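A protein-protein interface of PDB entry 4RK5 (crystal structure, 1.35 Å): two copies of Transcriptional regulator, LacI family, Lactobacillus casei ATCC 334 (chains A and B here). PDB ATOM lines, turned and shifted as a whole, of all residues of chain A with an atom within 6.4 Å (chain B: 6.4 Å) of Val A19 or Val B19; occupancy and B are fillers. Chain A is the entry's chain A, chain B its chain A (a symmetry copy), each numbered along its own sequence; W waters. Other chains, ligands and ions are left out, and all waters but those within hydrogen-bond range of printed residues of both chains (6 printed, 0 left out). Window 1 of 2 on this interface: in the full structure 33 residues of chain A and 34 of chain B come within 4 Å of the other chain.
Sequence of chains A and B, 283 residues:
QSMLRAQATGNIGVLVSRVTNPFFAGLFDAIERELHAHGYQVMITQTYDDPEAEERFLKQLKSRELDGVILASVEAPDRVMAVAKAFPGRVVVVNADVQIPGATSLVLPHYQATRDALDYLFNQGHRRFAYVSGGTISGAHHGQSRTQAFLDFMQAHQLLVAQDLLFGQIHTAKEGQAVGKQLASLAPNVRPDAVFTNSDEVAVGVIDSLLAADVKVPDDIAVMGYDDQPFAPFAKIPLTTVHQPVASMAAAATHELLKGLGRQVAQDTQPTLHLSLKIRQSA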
ATOM      1  N   VAL A  16     -10.657   1.919  35.498  1.00  0.00           N
ATOM      2  CA  VAL A  16     -11.691   0.967  35.176  1.00  0.00           C
ATOM      3  C   VAL A  16     -11.137  -0.079  34.184  1.00  0.00           C
ATOM      4  O   VAL A  16     -10.118   0.152  33.596  1.00  0.00           O
ATOM      5  CB  VAL A  16     -12.925   1.625  34.529  1.00  0.00           C
ATOM      6  CG1 VAL A  16     -13.507   2.679  35.463  1.00  0.00           C
ATOM      7  CG2 VAL A  16     -12.611   2.231  33.182  1.00  0.00           C
ATOM      8  N   SER A  17     -11.799  -1.200  34.010  1.00  0.00           N
ATOM      9  CA  SER A  17     -11.366  -2.116  32.968  1.00  0.00           C
ATOM     10  C   SER A  17     -11.616  -1.654  31.519  1.00  0.00           C
ATOM     11  O   SER A  17     -10.821  -1.931  30.660  1.00  0.00           O
ATOM     12  CB  SER A  17     -11.808  -3.547  33.250  1.00  0.00           C
ATOM     13  OG  SER A  17     -13.185  -3.663  33.132  1.00  0.00           O
ATOM     14  N   ARG A  18     -12.738  -0.983  31.261  1.00  0.00           N
ATOM     15  CA  ARG A  18     -13.124  -0.647  29.861  1.00  0.00           C
ATOM     16  C   ARG A  18     -14.091   0.519  29.858  1.00  0.00           C
ATOM     17  O   ARG A  18     -15.173   0.413  30.426  1.00  0.00           O
ATOM     18  CB  ARG A  18     -13.706  -1.875  29.183  1.00  0.00           C
ATOM     19  CG  ARG A  18     -14.154  -1.635  27.754  1.00  0.00           C
ATOM     20  CD  ARG A  18     -14.528  -2.937  27.024  1.00  0.00           C
ATOM     21  NE  ARG A  18     -15.536  -3.672  27.697  1.00  0.00           N
ATOM     22  CZ  ARG A  18     -16.856  -3.530  27.522  1.00  0.00           C
ATOM     23  NH1 ARG A  18     -17.368  -2.694  26.631  1.00  0.00           N
ATOM     24  NH2 ARG A  18     -17.670  -4.288  28.238  1.00  0.00           N
ATOM     25  N   VAL A  19     -13.715   1.616  29.199  1.00  0.00           N
ATOM     26  CA  VAL A  19     -14.533   2.794  29.125  1.00  0.00           C
ATOM     27  C   VAL A  19     -15.764   2.620  28.220  1.00  0.00           C
ATOM     28  O   VAL A  19     -16.753   3.354  28.433  1.00  0.00           O
ATOM     29  CB  VAL A  19     -13.655   4.017  28.748  1.00  0.00           C
ATOM     30  CG1 VAL A  19     -14.449   5.225  28.366  1.00  0.00           C
ATOM     31  CG2 VAL A  19     -12.713   4.343  29.881  1.00  0.00           C
ATOM     32  N   THR A  20     -15.724   1.729  27.235  1.00  0.00           N
ATOM     33  CA  THR A  20     -16.888   1.504  26.400  1.00  0.00           C
ATOM     34  C   THR A  20     -17.940   0.629  27.114  1.00  0.00           C
ATOM     35  O   THR A  20     -18.986   0.308  26.490  1.00  0.00           O
ATOM     36  CB  THR A  20     -16.496   0.844  25.081  1.00  0.00           C
ATOM     37  OG1 THR A  20     -15.821  -0.392  25.362  1.00  0.00           O
ATOM     38  CG2 THR A  20     -15.672   1.765  24.221  1.00  0.00           C
ATOM     39  N   ASN A  21     -17.687   0.218  28.353  1.00  0.00           N
ATOM     40  CA  ASN A  21     -18.748  -0.369  29.172  1.00  0.00           C
ATOM     41  C   ASN A  21     -19.563   0.803  29.726  1.00  0.00           C
ATOM     42  O   ASN A  21     -19.025   1.601  30.527  1.00  0.00           O
ATOM     43  CB  ASN A  21     -18.115  -1.173  30.302  1.00  0.00           C
ATOM     44  CG  ASN A  21     -19.110  -1.771  31.222  1.00  0.00           C
ATOM     45  OD1 ASN A  21     -20.251  -1.311  31.313  1.00  0.00           O
ATOM     46  ND2 ASN A  21     -18.671  -2.736  31.992  1.00  0.00           N
ATOM     47  N   PRO A  22     -20.867   0.948  29.345  1.00  0.00           N
ATOM     48  CA  PRO A  22     -21.603   2.128  29.783  1.00  0.00           C
ATOM     49  C   PRO A  22     -21.719   2.245  31.302  1.00  0.00           C
ATOM     50  O   PRO A  22     -21.993   3.344  31.777  1.00  0.00           O
ATOM     51  CB  PRO A  22     -22.955   1.964  29.108  1.00  0.00           C
ATOM     52  CG  PRO A  22     -22.622   1.129  27.886  1.00  0.00           C
ATOM     53  CD  PRO A  22     -21.614   0.141  28.358  1.00  0.00           C
ATOM     54  N   PHE A  24     -19.234   1.738  33.396  1.00  0.00           N
ATOM     55  CA  PHE A  24     -18.050   2.478  33.815  1.00  0.00           C
ATOM     56  C   PHE A  24     -18.082   3.917  33.301  1.00  0.00           C
ATOM     57  O   PHE A  24     -17.643   4.813  34.030  1.00  0.00           O
ATOM     58  CB  PHE A  24     -16.778   1.767  33.347  1.00  0.00           C
ATOM     59  CG  PHE A  24     -16.362   0.562  34.153  1.00  0.00           C
ATOM     60  CD1 PHE A  24     -16.317   0.613  35.537  1.00  0.00           C
ATOM     61  CD2 PHE A  24     -15.998  -0.618  33.540  1.00  0.00           C
ATOM     62  CE1 PHE A  24     -15.861  -0.457  36.272  1.00  0.00           C
ATOM     63  CE2 PHE A  24     -15.557  -1.707  34.297  1.00  0.00           C
ATOM     64  CZ  PHE A  24     -15.489  -1.593  35.660  1.00  0.00           C
ATOM     65  N   ALA A  25     -18.559   4.149  32.089  1.00  0.00           N
ATOM     66  CA  ALA A  25     -18.640   5.533  31.618  1.00  0.00           C
ATOM     67  C   ALA A  25     -19.541   6.359  32.530  1.00  0.00           C
ATOM     68  O   ALA A  25     -19.247   7.505  32.866  1.00  0.00           O
ATOM     69  CB  ALA A  25     -19.086   5.576  30.160  1.00  0.00           C
ATOM     70  N   GLY A  26     -20.692   5.768  32.913  1.00  0.00           N
ATOM     71  CA  GLY A  26     -21.625   6.463  33.777  1.00  0.00           C
ATOM     72  C   GLY A  26     -21.075   6.696  35.181  1.00  0.00           C
ATOM     73  O   GLY A  26     -21.295   7.768  35.788  1.00  0.00           O
ATOM     74  N   PHE A  28     -17.874   6.949  35.981  1.00  0.00           N
ATOM     75  CA  PHE A  28     -16.897   8.010  35.804  1.00  0.00           C
ATOM     76  C   PHE A  28     -17.578   9.388  35.746  1.00  0.00           C
ATOM     77  O   PHE A  28     -17.140  10.359  36.356  1.00  0.00           O
ATOM     78  CB  PHE A  28     -16.098   7.795  34.523  1.00  0.00           C
ATOM     79  CG  PHE A  28     -15.258   8.972  34.163  1.00  0.00           C
ATOM     80  CD1 PHE A  28     -14.150   9.308  34.895  1.00  0.00           C
ATOM     81  CD2 PHE A  28     -15.664   9.785  33.084  1.00  0.00           C
ATOM     82  CE1 PHE A  28     -13.408  10.473  34.554  1.00  0.00           C
ATOM     83  CE2 PHE A  28     -14.920  10.895  32.736  1.00  0.00           C
ATOM     84  CZ  PHE A  28     -13.830  11.223  33.498  1.00  0.00           C
ATOM     85  N   ASP A  29     -18.629   9.486  34.949  1.00  0.00           N
ATOM     86  CA  ASP A  29     -19.272  10.780  34.729  1.00  0.00           C
ATOM     87  C   ASP A  29     -19.779  11.321  36.078  1.00  0.00           C
ATOM     88  O   ASP A  29     -19.620  12.503  36.384  1.00  0.00           O
ATOM     89  CB  ASP A  29     -20.406  10.607  33.757  1.00  0.00           C
ATOM     90  CG  ASP A  29     -21.130  11.886  33.409  1.00  0.00           C
ATOM     91  OD1 ASP A  29     -20.491  12.855  32.924  1.00  0.00           O
ATOM     92  OD2 ASP A  29     -22.381  11.928  33.541  1.00  0.00           O
ATOM     93  N   ILE A  44      -9.535   9.456  33.382  1.00  0.00           N
ATOM     94  CA  ILE A  44      -9.795   7.987  33.458  1.00  0.00           C
ATOM     95  C   ILE A  44      -8.879   7.258  32.520  1.00  0.00           C
ATOM     96  O   ILE A  44      -8.597   7.716  31.384  1.00  0.00           O
ATOM     97  CB  ILE A  44     -11.293   7.686  33.292  1.00  0.00           C
ATOM     98  CG1 ILE A  44     -11.615   6.236  33.412  1.00  0.00           C
ATOM     99  CG2 ILE A  44     -11.900   8.304  32.072  1.00  0.00           C
ATOM    100  CD1 ILE A  44     -13.085   5.967  33.628  1.00  0.00           C
ATOM    101  N   THR A  45      -8.441   6.079  32.980  1.00  0.00           N
ATOM    102  CA  THR A  45      -7.641   5.108  32.232  1.00  0.00           C
ATOM    103  C   THR A  45      -8.356   3.771  32.298  1.00  0.00           C
ATOM    104  O   THR A  45      -9.008   3.460  33.292  1.00  0.00           O
ATOM    105  CB  THR A  45      -6.234   5.064  32.963  1.00  0.00           C
ATOM    106  OG1 THR A  45      -5.569   6.335  32.726  1.00  0.00           O
ATOM    107  CG2 THR A  45      -5.374   4.007  32.560  1.00  0.00           C
ATOM    108  N   GLN A  46      -8.164   2.983  31.257  1.00  0.00           N
ATOM    109  CA  GLN A  46      -8.692   1.625  31.229  1.00  0.00           C
ATOM    110  C   GLN A  46      -7.574   0.575  31.212  1.00  0.00           C
ATOM    111  O   GLN A  46      -6.532   0.811  30.609  1.00  0.00           O
ATOM    112  CB  GLN A  46      -9.642   1.413  30.041  1.00  0.00           C
ATOM    113  CG  GLN A  46      -9.041   1.701  28.656  1.00  0.00           C
ATOM    114  CD  GLN A  46     -10.047   1.568  27.546  1.00  0.00           C
ATOM    115  OE1 GLN A  46     -11.275   1.567  27.803  1.00  0.00           O
ATOM    116  NE2 GLN A  46      -9.598   1.497  26.299  1.00  0.00           N
ATOM    117  N   TYR A  48      -8.189  -3.065  30.593  1.00  0.00           N
ATOM    118  CA  TYR A  48      -8.449  -4.337  29.923  1.00  0.00           C
ATOM    119  C   TYR A  48      -7.960  -5.526  30.722  1.00  0.00           C
ATOM    120  O   TYR A  48      -7.475  -6.539  30.169  1.00  0.00           O
ATOM    121  CB  TYR A  48      -7.950  -4.319  28.499  1.00  0.00           C
ATOM    122  CG  TYR A  48      -8.949  -3.738  27.508  1.00  0.00           C
ATOM    123  CD1 TYR A  48      -9.005  -2.415  27.220  1.00  0.00           C
ATOM    124  CD2 TYR A  48      -9.869  -4.548  26.873  1.00  0.00           C
ATOM    125  CE1 TYR A  48      -9.885  -1.923  26.297  1.00  0.00           C
ATOM    126  CE2 TYR A  48     -10.768  -4.037  25.986  1.00  0.00           C
ATOM    127  CZ  TYR A  48     -10.769  -2.714  25.676  1.00  0.00           C
ATOM    128  OH  TYR A  48     -11.685  -2.258  24.776  1.00  0.00           O
ATOM    129  N   VAL B  16     -12.355  15.150  25.261  1.00  0.00           N
ATOM    130  CA  VAL B  16     -13.649  15.067  24.632  1.00  0.00           C
ATOM    131  C   VAL B  16     -14.666  15.908  25.436  1.00  0.00           C
ATOM    132  O   VAL B  16     -14.391  16.251  26.552  1.00  0.00           O
ATOM    133  CB  VAL B  16     -14.184  13.623  24.558  1.00  0.00           C
ATOM    134  CG1 VAL B  16     -13.210  12.743  23.784  1.00  0.00           C
ATOM    135  CG2 VAL B  16     -14.449  13.040  25.924  1.00  0.00           C
ATOM    136  N   SER B  17     -15.810  16.227  24.873  1.00  0.00           N
ATOM    137  CA  SER B  17     -16.827  16.883  25.676  1.00  0.00           C
ATOM    138  C   SER B  17     -17.510  16.007  26.745  1.00  0.00           C
ATOM    139  O   SER B  17     -17.834  16.493  27.796  1.00  0.00           O
ATOM    140  CB  SER B  17     -17.796  17.687  24.819  1.00  0.00           C
ATOM    141  OG  SER B  17     -18.586  16.842  24.053  1.00  0.00           O
ATOM    142  N   ARG B  18     -17.751  14.730  26.447  1.00  0.00           N
ATOM    143  CA  ARG B  18     -18.550  13.868  27.363  1.00  0.00           C
ATOM    144  C   ARG B  18     -18.244  12.409  27.096  1.00  0.00           C
ATOM    145  O   ARG B  18     -18.478  11.930  25.991  1.00  0.00           O
ATOM    146  CB  ARG B  18     -20.028  14.181  27.200  1.00  0.00           C
ATOM    147  CG  ARG B  18     -20.935  13.339  28.076  1.00  0.00           C
ATOM    148  CD  ARG B  18     -22.395  13.828  28.058  1.00  0.00           C
ATOM    149  NE  ARG B  18     -22.940  13.872  26.751  1.00  0.00           N
ATOM    150  CZ  ARG B  18     -23.569  12.865  26.131  1.00  0.00           C
ATOM    151  NH1 ARG B  18     -23.797  11.701  26.719  1.00  0.00           N
ATOM    152  NH2 ARG B  18     -24.014  13.064  24.901  1.00  0.00           N
ATOM    153  N   VAL B  19     -17.749  11.699  28.110  1.00  0.00           N
ATOM    154  CA  VAL B  19     -17.407  10.309  27.991  1.00  0.00           C
ATOM    155  C   VAL B  19     -18.636   9.391  27.892  1.00  0.00           C
ATOM    156  O   VAL B  19     -18.492   8.282  27.334  1.00  0.00           O
ATOM    157  CB  VAL B  19     -16.428   9.911  29.125  1.00  0.00           C
ATOM    158  CG1 VAL B  19     -16.240   8.434  29.260  1.00  0.00           C
ATOM    159  CG2 VAL B  19     -15.097  10.594  28.921  1.00  0.00           C
ATOM    160  N   THR B  20     -19.788   9.788  28.423  1.00  0.00           N
ATOM    161  CA  THR B  20     -20.977   8.968  28.298  1.00  0.00           C
ATOM    162  C   THR B  20     -21.611   9.095  26.896  1.00  0.00           C
ATOM    163  O   THR B  20     -22.680   8.476  26.656  1.00  0.00           O
ATOM    164  CB  THR B  20     -22.013   9.342  29.353  1.00  0.00           C
ATOM    165  OG1 THR B  20     -22.335  10.735  29.217  1.00  0.00           O
ATOM    166  CG2 THR B  20     -21.544   8.995  30.741  1.00  0.00           C
ATOM    167  N   ASN B  21     -21.019   9.881  26.001  1.00  0.00           N
ATOM    168  CA  ASN B  21     -21.406   9.825  24.592  1.00  0.00           C
ATOM    169  C   ASN B  21     -20.692   8.608  23.997  1.00  0.00           C
ATOM    170  O   ASN B  21     -19.441   8.604  23.925  1.00  0.00           O
ATOM    171  CB  ASN B  21     -20.957  11.109  23.903  1.00  0.00           C
ATOM    172  CG  ASN B  21     -21.261  11.130  22.453  1.00  0.00           C
ATOM    173  OD1 ASN B  21     -21.439  10.085  21.824  1.00  0.00           O
ATOM    174  ND2 ASN B  21     -21.224  12.307  21.878  1.00  0.00           N
ATOM    175  N   PRO B  22     -21.433   7.554  23.542  1.00  0.00           N
ATOM    176  CA  PRO B  22     -20.746   6.353  23.085  1.00  0.00           C
ATOM    177  C   PRO B  22     -19.815   6.598  21.899  1.00  0.00           C
ATOM    178  O   PRO B  22     -18.942   5.765  21.668  1.00  0.00           O
ATOM    179  CB  PRO B  22     -21.888   5.409  22.742  1.00  0.00           C
ATOM    180  CG  PRO B  22     -23.007   5.895  23.643  1.00  0.00           C
ATOM    181  CD  PRO B  22     -22.898   7.380  23.627  1.00  0.00           C
ATOM    182  N   PHE B  24     -17.732   9.133  21.668  1.00  0.00           N
ATOM    183  CA  PHE B  24     -16.447   9.490  22.258  1.00  0.00           C
ATOM    184  C   PHE B  24     -15.832   8.310  23.008  1.00  0.00           C
ATOM    185  O   PHE B  24     -14.609   8.152  22.959  1.00  0.00           O
ATOM    186  CB  PHE B  24     -16.597  10.699  23.183  1.00  0.00           C
ATOM    187  CG  PHE B  24     -16.705  12.041  22.503  1.00  0.00           C
ATOM    188  CD1 PHE B  24     -15.822  12.402  21.498  1.00  0.00           C
ATOM    189  CD2 PHE B  24     -17.671  12.954  22.870  1.00  0.00           C
ATOM    190  CE1 PHE B  24     -15.866  13.655  20.930  1.00  0.00           C
ATOM    191  CE2 PHE B  24     -17.721  14.216  22.272  1.00  0.00           C
ATOM    192  CZ  PHE B  24     -16.799  14.542  21.314  1.00  0.00           C
ATOM    193  N   ALA B  25     -16.629   7.512  23.701  1.00  0.00           N
ATOM    194  CA  ALA B  25     -16.047   6.350  24.375  1.00  0.00           C
ATOM    195  C   ALA B  25     -15.385   5.419  23.367  1.00  0.00           C
ATOM    196  O   ALA B  25     -14.299   4.885  23.594  1.00  0.00           O
ATOM    197  CB  ALA B  25     -17.100   5.642  25.223  1.00  0.00           C
ATOM    198  N   GLY B  26     -16.077   5.190  22.232  1.00  0.00           N
ATOM    199  CA  GLY B  26     -15.543   4.319  21.205  1.00  0.00           C
ATOM    200  C   GLY B  26     -14.294   4.885  20.535  1.00  0.00           C
ATOM    201  O   GLY B  26     -13.335   4.141  20.229  1.00  0.00           O
ATOM    202  N   PHE B  28     -12.158   7.002  21.914  1.00  0.00           N
ATOM    203  CA  PHE B  28     -11.117   6.837  22.913  1.00  0.00           C
ATOM    204  C   PHE B  28     -10.571   5.398  22.916  1.00  0.00           C
ATOM    205  O   PHE B  28      -9.370   5.156  22.976  1.00  0.00           O
ATOM    206  CB  PHE B  28     -11.651   7.169  24.303  1.00  0.00           C
ATOM    207  CG  PHE B  28     -10.707   6.785  25.390  1.00  0.00           C
ATOM    208  CD1 PHE B  28      -9.533   7.462  25.590  1.00  0.00           C
ATOM    209  CD2 PHE B  28     -11.013   5.655  26.179  1.00  0.00           C
ATOM    210  CE1 PHE B  28      -8.632   7.027  26.601  1.00  0.00           C
ATOM    211  CE2 PHE B  28     -10.151   5.259  27.182  1.00  0.00           C
ATOM    212  CZ  PHE B  28      -8.972   5.939  27.346  1.00  0.00           C
ATOM    213  N   ASP B  29     -11.475   4.433  22.916  1.00  0.00           N
ATOM    214  CA  ASP B  29     -11.063   3.036  23.041  1.00  0.00           C
ATOM    215  C   ASP B  29     -10.141   2.680  21.862  1.00  0.00           C
ATOM    216  O   ASP B  29      -9.113   2.025  22.040  1.00  0.00           O
ATOM    217  CB  ASP B  29     -12.287   2.163  23.051  1.00  0.00           C
ATOM    218  CG  ASP B  29     -12.000   0.688  23.221  1.00  0.00           C
ATOM    219  OD1 ASP B  29     -11.361   0.287  24.228  1.00  0.00           O
ATOM    220  OD2 ASP B  29     -12.477  -0.121  22.384  1.00  0.00           O
ATOM    221  N   ILE B  44      -8.189   9.960  29.535  1.00  0.00           N
ATOM    222  CA  ILE B  44      -9.222  10.854  28.931  1.00  0.00           C
ATOM    223  C   ILE B  44      -9.830  11.721  29.995  1.00  0.00           C
ATOM    224  O   ILE B  44     -10.080  11.277  31.144  1.00  0.00           O
ATOM    225  CB  ILE B  44     -10.216  10.049  28.080  1.00  0.00           C
ATOM    226  CG1 ILE B  44     -11.238  10.902  27.411  1.00  0.00           C
ATOM    227  CG2 ILE B  44     -10.827   8.891  28.803  1.00  0.00           C
ATOM    228  CD1 ILE B  44     -11.970  10.194  26.296  1.00  0.00           C
ATOM    229  N   THR B  45     -10.118  12.966  29.596  1.00  0.00           N
ATOM    230  CA  THR B  45     -10.825  13.979  30.382  1.00  0.00           C
ATOM    231  C   THR B  45     -11.990  14.480  29.549  1.00  0.00           C
ATOM    232  O   THR B  45     -11.902  14.541  28.325  1.00  0.00           O
ATOM    233  CB  THR B  45      -9.760  15.120  30.660  1.00  0.00           C
ATOM    234  OG1 THR B  45      -8.763  14.587  31.575  1.00  0.00           O
ATOM    235  CG2 THR B  45     -10.288  16.324  31.199  1.00  0.00           C
ATOM    236  N   GLN B  46     -13.036  14.889  30.242  1.00  0.00           N
ATOM    237  CA  GLN B  46     -14.185  15.503  29.586  1.00  0.00           C
ATOM    238  C   GLN B  46     -14.356  16.973  29.988  1.00  0.00           C
ATOM    239  O   GLN B  46     -14.078  17.323  31.130  1.00  0.00           O
ATOM    240  CB  GLN B  46     -15.477  14.719  29.859  1.00  0.00           C
ATOM    241  CG  GLN B  46     -15.838  14.538  31.341  1.00  0.00           C
ATOM    242  CD  GLN B  46     -17.058  13.683  31.542  1.00  0.00           C
ATOM    243  OE1 GLN B  46     -17.478  12.952  30.614  1.00  0.00           O
ATOM    244  NE2 GLN B  46     -17.640  13.695  32.735  1.00  0.00           N
ATOM    245  N   TYR B  48     -17.384  18.995  29.121  1.00  0.00           N
ATOM    246  CA  TYR B  48     -18.735  19.552  29.133  1.00  0.00           C
ATOM    247  C   TYR B  48     -18.803  20.928  28.506  1.00  0.00           C
ATOM    248  O   TYR B  48     -19.567  21.817  28.945  1.00  0.00           O
ATOM    249  CB  TYR B  48     -19.343  19.486  30.513  1.00  0.00           C
ATOM    250  CG  TYR B  48     -20.024  18.159  30.818  1.00  0.00           C
ATOM    251  CD1 TYR B  48     -19.361  17.106  31.354  1.00  0.00           C
ATOM    252  CD2 TYR B  48     -21.360  17.967  30.533  1.00  0.00           C
ATOM    253  CE1 TYR B  48     -20.004  15.938  31.655  1.00  0.00           C
ATOM    254  CE2 TYR B  48     -21.978  16.782  30.801  1.00  0.00           C
ATOM    255  CZ  TYR B  48     -21.303  15.759  31.386  1.00  0.00           C
ATOM    256  OH  TYR B  48     -21.972  14.599  31.639  1.00  0.00           O
HETATM  257  O   HOH W   1     -23.804  14.194  34.565  1.00  0.00           O
HETATM  258  O   HOH W   2     -14.755  -1.689  23.281  1.00  0.00           O
HETATM  259  O   HOH W   3     -23.928  11.797  31.083  1.00  0.00           O
HETATM  260  O   HOH W   4     -11.053  -2.386  21.359  1.00  0.00           O
HETATM  261  O   HOH W   5     -13.181   1.206  26.149  1.00  0.00           O
HETATM  262  O   HOH W   6     -19.591  11.527  30.627  1.00  0.00           O
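The side-chain amide nitrogen (NE2) of Gln A46 is in hydrogen-bond range of the side-chain carboxylate (OD1) of Asp B29.
The side-chain amide nitrogen (NE2) of Gln B46 sits at hydrogen-bond distance from the side-chain carboxylate (OD1) of Asp A29 (3.0 Å).
The side-chain hydroxyl (OH) of Tyr A48 sits at hydrogen-bond distance from the side-chain carboxylate (OD1) of Asp B29 (2.6 Å).
O of Ile A44 is in hydrogen-bond range of N of Ile B44, at 2.9 Å.
OD1 of Asp A29 lies within hydrogen-bond range of OH of Tyr B48, 2.6 Å away.
The backbone carbonyl oxygen (O) of Ser A17 sits at hydrogen-bond distance from the backbone NH (N) of Tyr A48, 2.9 Å away.
The backbone NH of Val A19 is in hydrogen-bond range of the side-chain amide oxygen of Gln A46 (2.8 Å).
The guanidinium group (NH1) of Arg B18 is in hydrogen-bond range of the side-chain hydroxyl (OG1) of Thr B20 (3.1 Å).
The guanidinium group of Arg A18 is in hydrogen-bond range of the side-chain hydroxyl of Thr A20, at 3.1 Å.
The backbone carbonyl oxygen of Ser B17 is in hydrogen-bond range of the backbone NH of Tyr B48 (2.9 Å).
OE1 of Gln B46 sits at hydrogen-bond distance from N of Val B19, at 2.8 Å.
Val A19 touches Ala B25.
Phe B28 touches Val A19 (CE2 to CG2, 3.8 Å).
CA of Gly B26 touches CG2 of Thr A20 (3.95 Å).
Asp B29 touches Thr A20 (CB to CG2, 3.6 Å).
CB of Ala A25 touches O of Val B19, 3.96 Å away.
Thr B20 touches Gly A26 (CG2 to CA, 3.95 Å).
Phe A28 touches Val B19 (CE2 to CG2, 3.8 Å).
CD of Gln B46 touches CE2 of Phe A28 (3.7 Å).
Thr B20 touches Asp A29.
Gln A46 touches Phe B28 (CD to CE2, 3.7 Å).
Of chain B, only Val B19 (3.8 Å), Ala B25 (3.96 Å) and Phe B28 (3.8 Å) come within 4 Å of Val A19.
Printed residues of chain B within 4 Å of Phe A28: Val B19 (3.8 Å) and Gln B46 (3.7 Å).
Of chain A, only Val A19 (3.8 Å), Ala A25 (3.96 Å) and Phe A28 (3.8 Å) come within 4 Å of Val B19.
Of the printed residues of chain A, Phe B28 touches Val A19 and Gln A46.
Of the printed residues of chain A, Asp B29 touches Thr A20, Gln A46 and Tyr A48.
The nearest residue of chain B that does not touch Val A19 is Ile B44 (5.0 Å).
Of the 16 printed residues of chain A, 9 touch a printed residue of chain B.
Hydrophobic or aromatic side chains of chain A within 4 Å of the printed part of chain B: Val A19, Ala A25, Phe A28, Ile A44 and Tyr A48.
Hydrophobic or aromatic side chains of chain B within 4 Å of the printed part of chain A: Val B19, Ala B25, Phe B28, Ile B44 and Tyr B48.
Among the printed residues, 18 pairs touch across the chains.
Among the printed residues, no Asp or Glu carboxylate lies within 4 Å of a Lys or Arg side-chain nitrogen of the other chain.
Val A19 touches Ala B25, and with the chains exchanged Ala A25 touches Val B19.
Thr A20 touches Ala B25, and with the chains exchanged Ala A25 touches Thr B20.
Thr A20 touches Asp B29, and with the chains exchanged Asp A29 touches Thr B20.
Asp A29 touches Gln B46, and with the chains exchanged Gln A46 touches Asp B29.
Water W6 lies within hydrogen-bond range of OE1 of Gln B46 (2.5 Å), OD1 of Asp A29 (2.8 Å), N of Thr B20 (2.8 Å) and N of Val B19 (3.1 Å).
Water W5 lies within hydrogen-bond range of the side-chain amide oxygen of Gln A46 (2.5 Å), the side-chain carboxylate of Asp B29 (2.8 Å), the backbone NH of Thr A20 (2.8 Å) and the backbone NH of Val A19 (3.1 Å).
Water W2 lies within hydrogen-bond range of OG1 of Thr A20 (2.7 Å), OD2 of Asp B29 (2.9 Å) and OH of Tyr A48 (3.5 Å).
Water W3 lies within hydrogen-bond range of the side-chain hydroxyl of Thr B20 (2.7 Å), the side-chain carboxylate of Asp A29 (2.9 Å) and the side-chain hydroxyl of Tyr B48 (3.5 Å).
Water W4 bridges OD2 of Asp B29 (2.9 Å) and OH of Tyr A48 (3.5 Å).
Water W1 lies within hydrogen-bond range of the side-chain carboxylate of Asp A29 and the side-chain hydroxyl of Tyr B48.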
